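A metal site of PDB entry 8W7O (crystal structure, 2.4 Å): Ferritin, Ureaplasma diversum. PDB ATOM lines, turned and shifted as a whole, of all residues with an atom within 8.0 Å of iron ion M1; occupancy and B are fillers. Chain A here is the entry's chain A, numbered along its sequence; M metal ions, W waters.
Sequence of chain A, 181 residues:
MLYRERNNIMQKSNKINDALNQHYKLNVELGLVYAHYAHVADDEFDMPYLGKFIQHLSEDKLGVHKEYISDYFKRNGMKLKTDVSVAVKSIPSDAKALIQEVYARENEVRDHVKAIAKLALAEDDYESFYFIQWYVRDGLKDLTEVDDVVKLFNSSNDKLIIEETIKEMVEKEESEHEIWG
Water W1 lies within hydrogen-bond range of OD1 of Asp 60 (2.9 Å), OD1 of Asp 138 (2.9 Å) and NZ of Lys 141 (3.0 Å).
Iron ion M1 is bound by OD2 of Asp 138, OD2 of Asp 60, NE2 of His 65, OD2 of Asp 142 and water W1.
ND1 of His 65 lies close to OD1 of Asn 27, 3.3 Å away. The side-chain carboxylate (OD1) of Asp 142 is in salt-bridge range of the side-chain amino group (NZ) of Lys 141, 2.7 Å away. OD2 of Asp 142 lies close to NZ of Lys 61 (3.1 Å). The side-chain hydroxyl (OH) of Tyr 135 is in hydrogen-bond range of the backbone carbonyl oxygen (O) of His 65, at 2.8 Å. The side-chain carboxylate of Asp 138 lies within salt-bridge range of the side-chain amino group of Lys 141 (2.7 Å).
Residues that only touch iron ion M1: Lys 141 (3.4 Å). Five residues have an atom within 4 Å of iron ion M1: Asp 60, His 65, Asp 138, Lys 141 and Asp 142. The nearest printed residue that does not touch iron ion M1 is Trp 134 (4.4 Å).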
ATOM      1  N   ASN A  27      -0.318   4.181 -22.586  1.00  0.00           N
ATOM      2  CA  ASN A  27       0.172   3.016 -23.313  1.00  0.00           C
ATOM      3  C   ASN A  27       1.647   3.144 -23.670  1.00  0.00           C
ATOM      4  O   ASN A  27       2.365   2.138 -23.643  1.00  0.00           O
ATOM      5  CB  ASN A  27      -0.651   2.762 -24.571  1.00  0.00           C
ATOM      6  CG  ASN A  27      -1.933   2.002 -24.256  1.00  0.00           C
ATOM      7  OD1 ASN A  27      -1.896   0.807 -23.954  1.00  0.00           O
ATOM      8  ND2 ASN A  27      -3.071   2.699 -24.283  1.00  0.00           N
ATOM      9  N   HIS A  56       6.136  -9.123 -25.410  1.00  0.00           N
ATOM     10  CA  HIS A  56       5.017  -9.073 -26.343  1.00  0.00           C
ATOM     11  C   HIS A  56       3.969  -8.058 -25.884  1.00  0.00           C
ATOM     12  O   HIS A  56       3.451  -7.283 -26.689  1.00  0.00           O
ATOM     13  CB  HIS A  56       4.388 -10.459 -26.505  1.00  0.00           C
ATOM     14  CG  HIS A  56       3.240 -10.489 -27.473  1.00  0.00           C
ATOM     15  ND1 HIS A  56       3.392 -10.872 -28.787  1.00  0.00           N
ATOM     16  CD2 HIS A  56       1.934 -10.170 -27.318  1.00  0.00           C
ATOM     17  CE1 HIS A  56       2.226 -10.791 -29.402  1.00  0.00           C
ATOM     18  NE2 HIS A  56       1.321 -10.373 -28.535  1.00  0.00           N
ATOM     19  N   LEU A  57       3.663  -8.048 -24.593  1.00  0.00           N
ATOM     20  CA  LEU A  57       2.713  -7.075 -24.064  1.00  0.00           C
ATOM     21  C   LEU A  57       3.243  -5.653 -24.214  1.00  0.00           C
ATOM     22  O   LEU A  57       2.490  -4.712 -24.487  1.00  0.00           O
ATOM     23  CB  LEU A  57       2.412  -7.411 -22.596  1.00  0.00           C
ATOM     24  CG  LEU A  57       1.239  -6.763 -21.860  1.00  0.00           C
ATOM     25  CD1 LEU A  57      -0.088  -6.958 -22.589  1.00  0.00           C
ATOM     26  CD2 LEU A  57       1.182  -7.303 -20.449  1.00  0.00           C
ATOM     27  N   GLU A  59       5.306  -4.519 -26.667  1.00  0.00           N
ATOM     28  CA  GLU A  59       5.145  -4.128 -28.066  1.00  0.00           C
ATOM     29  C   GLU A  59       3.675  -3.925 -28.422  1.00  0.00           C
ATOM     30  O   GLU A  59       3.365  -3.153 -29.335  1.00  0.00           O
ATOM     31  CB  GLU A  59       5.791  -5.176 -28.956  1.00  0.00           C
ATOM     32  CG  GLU A  59       7.293  -5.223 -28.729  1.00  0.00           C
ATOM     33  CD  GLU A  59       7.926  -6.491 -29.250  1.00  0.00           C
ATOM     34  OE1 GLU A  59       9.161  -6.600 -29.178  1.00  0.00           O
ATOM     35  OE2 GLU A  59       7.179  -7.368 -29.739  1.00  0.00           O
ATOM     36  N   ASP A  60       2.770  -4.613 -27.724  1.00  0.00           N
ATOM     37  CA  ASP A  60       1.347  -4.367 -27.895  1.00  0.00           C
ATOM     38  C   ASP A  60       0.974  -2.935 -27.462  1.00  0.00           C
ATOM     39  O   ASP A  60       0.320  -2.202 -28.208  1.00  0.00           O
ATOM     40  CB  ASP A  60       0.578  -5.420 -27.097  1.00  0.00           C
ATOM     41  CG  ASP A  60      -0.894  -5.373 -27.328  1.00  0.00           C
ATOM     42  OD1 ASP A  60      -1.305  -5.134 -28.490  1.00  0.00           O
ATOM     43  OD2 ASP A  60      -1.644  -5.570 -26.338  1.00  0.00           O
ATOM     44  N   LYS A  61       1.425  -2.514 -26.269  1.00  0.00           N
ATOM     45  CA  LYS A  61       1.068  -1.191 -25.745  1.00  0.00           C
ATOM     46  C   LYS A  61       1.694  -0.092 -26.576  1.00  0.00           C
ATOM     47  O   LYS A  61       1.076   0.964 -26.789  1.00  0.00           O
ATOM     48  CB  LYS A  61       1.520  -1.013 -24.284  1.00  0.00           C
ATOM     49  CG  LYS A  61       1.037  -2.065 -23.302  1.00  0.00           C
ATOM     50  CD  LYS A  61      -0.476  -2.058 -23.214  1.00  0.00           C
ATOM     51  CE  LYS A  61      -0.957  -2.976 -22.113  1.00  0.00           C
ATOM     52  NZ  LYS A  61      -2.432  -3.215 -22.177  1.00  0.00           N
ATOM     53  N   VAL A  64      -0.199  -1.083 -31.482  1.00  0.00           N
ATOM     54  CA  VAL A  64      -1.569  -0.806 -31.883  1.00  0.00           C
ATOM     55  C   VAL A  64      -2.306   0.001 -30.814  1.00  0.00           C
ATOM     56  O   VAL A  64      -3.141   0.854 -31.136  1.00  0.00           O
ATOM     57  CB  VAL A  64      -2.307  -2.120 -32.213  1.00  0.00           C
ATOM     58  CG1 VAL A  64      -1.618  -2.827 -33.378  1.00  0.00           C
ATOM     59  CG2 VAL A  64      -2.418  -3.023 -30.990  1.00  0.00           C
ATOM     60  N   HIS A  65      -2.021  -0.239 -29.535  1.00  0.00           N
ATOM     61  CA  HIS A  65      -2.703   0.504 -28.482  1.00  0.00           C
ATOM     62  C   HIS A  65      -2.524   2.013 -28.648  1.00  0.00           C
ATOM     63  O   HIS A  65      -3.466   2.776 -28.439  1.00  0.00           O
ATOM     64  CB  HIS A  65      -2.214   0.056 -27.105  1.00  0.00           C
ATOM     65  CG  HIS A  65      -2.883  -1.190 -26.618  1.00  0.00           C
ATOM     66  ND1 HIS A  65      -3.891  -1.165 -25.679  1.00  0.00           N
ATOM     67  CD2 HIS A  65      -2.668  -2.491 -26.922  1.00  0.00           C
ATOM     68  CE1 HIS A  65      -4.278  -2.411 -25.432  1.00  0.00           C
ATOM     69  NE2 HIS A  65      -3.548  -3.228 -26.166  1.00  0.00           N
ATOM     70  N   TYR A  68      -3.758   3.160 -32.928  1.00  0.00           N
ATOM     71  CA  TYR A  68      -5.178   3.323 -33.199  1.00  0.00           C
ATOM     72  C   TYR A  68      -5.677   4.701 -32.778  1.00  0.00           C
ATOM     73  O   TYR A  68      -6.512   5.304 -33.468  1.00  0.00           O
ATOM     74  CB  TYR A  68      -6.008   2.261 -32.473  1.00  0.00           C
ATOM     75  CG  TYR A  68      -5.800   0.856 -32.945  1.00  0.00           C
ATOM     76  CD1 TYR A  68      -5.420   0.592 -34.261  1.00  0.00           C
ATOM     77  CD2 TYR A  68      -5.998  -0.213 -32.090  1.00  0.00           C
ATOM     78  CE1 TYR A  68      -5.243  -0.711 -34.701  1.00  0.00           C
ATOM     79  CE2 TYR A  68      -5.820  -1.515 -32.521  1.00  0.00           C
ATOM     80  CZ  TYR A  68      -5.446  -1.759 -33.816  1.00  0.00           C
ATOM     81  OH  TYR A  68      -5.276  -3.050 -34.235  1.00  0.00           O
ATOM     82  N   GLU A 106      -2.674  -3.668 -15.629  1.00  0.00           N
ATOM     83  CA  GLU A 106      -3.680  -3.976 -16.641  1.00  0.00           C
ATOM     84  C   GLU A 106      -5.095  -3.811 -16.095  1.00  0.00           C
ATOM     85  O   GLU A 106      -6.009  -3.426 -16.831  1.00  0.00           O
ATOM     86  CB  GLU A 106      -3.502  -5.402 -17.180  1.00  0.00           C
ATOM     87  CG  GLU A 106      -2.210  -5.626 -17.940  1.00  0.00           C
ATOM     88  CD  GLU A 106      -2.089  -4.743 -19.154  1.00  0.00           C
ATOM     89  OE1 GLU A 106      -3.009  -4.751 -20.012  1.00  0.00           O
ATOM     90  OE2 GLU A 106      -1.093  -4.014 -19.249  1.00  0.00           O
ATOM     91  N   VAL A 109      -5.963  -0.302 -16.427  1.00  0.00           N
ATOM     92  CA  VAL A 109      -6.319  -0.002 -17.809  1.00  0.00           C
ATOM     93  C   VAL A 109      -7.818  -0.164 -18.012  1.00  0.00           C
ATOM     94  O   VAL A 109      -8.469   0.693 -18.630  1.00  0.00           O
ATOM     95  CB  VAL A 109      -5.512  -0.879 -18.784  1.00  0.00           C
ATOM     96  CG1 VAL A 109      -6.129  -0.876 -20.186  1.00  0.00           C
ATOM     97  CG2 VAL A 109      -4.051  -0.421 -18.834  1.00  0.00           C
ATOM     98  N   TRP A 134     -13.136  -1.500 -28.998  1.00  0.00           N
ATOM     99  CA  TRP A 134     -11.967  -2.363 -29.134  1.00  0.00           C
ATOM    100  C   TRP A 134     -11.144  -2.379 -27.850  1.00  0.00           C
ATOM    101  O   TRP A 134     -10.716  -3.439 -27.390  1.00  0.00           O
ATOM    102  CB  TRP A 134     -11.086  -1.907 -30.308  1.00  0.00           C
ATOM    103  CG  TRP A 134      -9.927  -2.830 -30.492  1.00  0.00           C
ATOM    104  CD1 TRP A 134      -9.913  -3.983 -31.237  1.00  0.00           C
ATOM    105  CD2 TRP A 134      -8.630  -2.738 -29.877  1.00  0.00           C
ATOM    106  NE1 TRP A 134      -8.690  -4.601 -31.132  1.00  0.00           N
ATOM    107  CE2 TRP A 134      -7.878  -3.858 -30.316  1.00  0.00           C
ATOM    108  CE3 TRP A 134      -8.025  -1.813 -29.017  1.00  0.00           C
ATOM    109  CZ2 TRP A 134      -6.556  -4.063 -29.931  1.00  0.00           C
ATOM    110  CZ3 TRP A 134      -6.712  -2.027 -28.620  1.00  0.00           C
ATOM    111  CH2 TRP A 134      -5.992  -3.146 -29.075  1.00  0.00           C
ATOM    112  N   TYR A 135     -10.924  -1.202 -27.257  1.00  0.00           N
ATOM    113  CA  TYR A 135     -10.192  -1.134 -26.003  1.00  0.00           C
ATOM    114  C   TYR A 135     -10.977  -1.776 -24.868  1.00  0.00           C
ATOM    115  O   TYR A 135     -10.381  -2.402 -23.995  1.00  0.00           O
ATOM    116  CB  TYR A 135      -9.871   0.312 -25.671  1.00  0.00           C
ATOM    117  CG  TYR A 135      -8.871   0.898 -26.611  1.00  0.00           C
ATOM    118  CD1 TYR A 135      -9.263   1.344 -27.860  1.00  0.00           C
ATOM    119  CD2 TYR A 135      -7.527   1.002 -26.255  1.00  0.00           C
ATOM    120  CE1 TYR A 135      -8.350   1.886 -28.748  1.00  0.00           C
ATOM    121  CE2 TYR A 135      -6.592   1.533 -27.125  1.00  0.00           C
ATOM    122  CZ  TYR A 135      -7.014   1.981 -28.371  1.00  0.00           C
ATOM    123  OH  TYR A 135      -6.110   2.534 -29.257  1.00  0.00           O
ATOM    124  N   ARG A 137     -12.916  -4.379 -25.054  1.00  0.00           N
ATOM    125  CA  ARG A 137     -12.728  -5.823 -25.120  1.00  0.00           C
ATOM    126  C   ARG A 137     -11.295  -6.215 -24.816  1.00  0.00           C
ATOM    127  O   ARG A 137     -11.052  -7.200 -24.101  1.00  0.00           O
ATOM    128  CB  ARG A 137     -13.147  -6.350 -26.497  1.00  0.00           C
ATOM    129  CG  ARG A 137     -12.955  -7.856 -26.662  1.00  0.00           C
ATOM    130  CD  ARG A 137     -13.724  -8.640 -25.577  1.00  0.00           C
ATOM    131  NE  ARG A 137     -13.392 -10.068 -25.551  1.00  0.00           N
ATOM    132  CZ  ARG A 137     -12.597 -10.644 -24.645  1.00  0.00           C
ATOM    133  NH1 ARG A 137     -12.361 -11.949 -24.709  1.00  0.00           N
ATOM    134  NH2 ARG A 137     -12.041  -9.914 -23.693  1.00  0.00           N
ATOM    135  N   ASP A 138     -10.323  -5.456 -25.332  1.00  0.00           N
ATOM    136  CA  ASP A 138      -8.923  -5.810 -25.145  1.00  0.00           C
ATOM    137  C   ASP A 138      -8.484  -5.653 -23.693  1.00  0.00           C
ATOM    138  O   ASP A 138      -7.544  -6.328 -23.258  1.00  0.00           O
ATOM    139  CB  ASP A 138      -8.038  -4.967 -26.056  1.00  0.00           C
ATOM    140  CG  ASP A 138      -6.649  -5.539 -26.166  1.00  0.00           C
ATOM    141  OD1 ASP A 138      -6.519  -6.643 -26.735  1.00  0.00           O
ATOM    142  OD2 ASP A 138      -5.702  -4.921 -25.657  1.00  0.00           O
ATOM    143  N   GLY A 139      -9.117  -4.750 -22.953  1.00  0.00           N
ATOM    144  CA  GLY A 139      -8.804  -4.617 -21.534  1.00  0.00           C
ATOM    145  C   GLY A 139      -8.988  -5.930 -20.786  1.00  0.00           C
ATOM    146  O   GLY A 139      -8.128  -6.321 -19.994  1.00  0.00           O
ATOM    147  N   LYS A 141      -9.091  -8.940 -22.295  1.00  0.00           N
ATOM    148  CA  LYS A 141      -8.203  -9.932 -22.906  1.00  0.00           C
ATOM    149  C   LYS A 141      -6.783  -9.847 -22.347  1.00  0.00           C
ATOM    150  O   LYS A 141      -6.213 -10.844 -21.907  1.00  0.00           O
ATOM    151  CB  LYS A 141      -8.220  -9.742 -24.431  1.00  0.00           C
ATOM    152  CG  LYS A 141      -7.536 -10.849 -25.244  1.00  0.00           C
ATOM    153  CD  LYS A 141      -6.659 -10.261 -26.350  1.00  0.00           C
ATOM    154  CE  LYS A 141      -5.445  -9.594 -25.746  1.00  0.00           C
ATOM    155  NZ  LYS A 141      -4.690  -8.623 -26.622  1.00  0.00           N
ATOM    156  N   ASP A 142      -6.196  -8.644 -22.358  1.00  0.00           N
ATOM    157  CA  ASP A 142      -4.837  -8.486 -21.834  1.00  0.00           C
ATOM    158  C   ASP A 142      -4.786  -8.860 -20.360  1.00  0.00           C
ATOM    159  O   ASP A 142      -3.846  -9.535 -19.925  1.00  0.00           O
ATOM    160  CB  ASP A 142      -4.351  -7.033 -22.028  1.00  0.00           C
ATOM    161  CG  ASP A 142      -3.877  -6.745 -23.468  1.00  0.00           C
ATOM    162  OD1 ASP A 142      -3.737  -7.694 -24.254  1.00  0.00           O
ATOM    163  OD2 ASP A 142      -3.627  -5.564 -23.808  1.00  0.00           O
ATOM    164  N   LEU A 143      -5.795  -8.439 -19.601  1.00  0.00           N
ATOM    165  CA  LEU A 143      -5.866  -8.818 -18.202  1.00  0.00           C
ATOM    166  C   LEU A 143      -5.943 -10.332 -18.029  1.00  0.00           C
ATOM    167  O   LEU A 143      -5.338 -10.888 -17.109  1.00  0.00           O
ATOM    168  CB  LEU A 143      -7.078  -8.160 -17.541  1.00  0.00           C
ATOM    169  CG  LEU A 143      -7.200  -8.535 -16.075  1.00  0.00           C
ATOM    170  CD1 LEU A 143      -6.282  -7.618 -15.296  1.00  0.00           C
ATOM    171  CD2 LEU A 143      -8.623  -8.411 -15.578  1.00  0.00           C
ATOM    172  N   GLU A 145      -4.887 -12.746 -20.186  1.00  0.00           N
ATOM    173  CA  GLU A 145      -3.612 -13.359 -20.533  1.00  0.00           C
ATOM    174  C   GLU A 145      -2.597 -13.178 -19.409  1.00  0.00           C
ATOM    175  O   GLU A 145      -1.857 -14.107 -19.083  1.00  0.00           O
ATOM    176  CB  GLU A 145      -3.074 -12.760 -21.846  1.00  0.00           C
ATOM    177  CG  GLU A 145      -3.872 -13.234 -23.053  1.00  0.00           C
ATOM    178  CD  GLU A 145      -3.524 -12.484 -24.325  1.00  0.00           C
ATOM    179  OE1 GLU A 145      -2.635 -11.606 -24.288  1.00  0.00           O
ATOM    180  OE2 GLU A 145      -4.150 -12.792 -25.366  1.00  0.00           O
HETATM  181 FE    FE M   1      -3.747  -5.377 -25.975  1.00  0.00          FE
HETATM  182 FE    FE M   2      -1.254 -10.651 -28.343  1.00  0.00          FE
HETATM  183  O   HOH W   1      -4.019  -6.123 -28.143  1.00  0.00           O
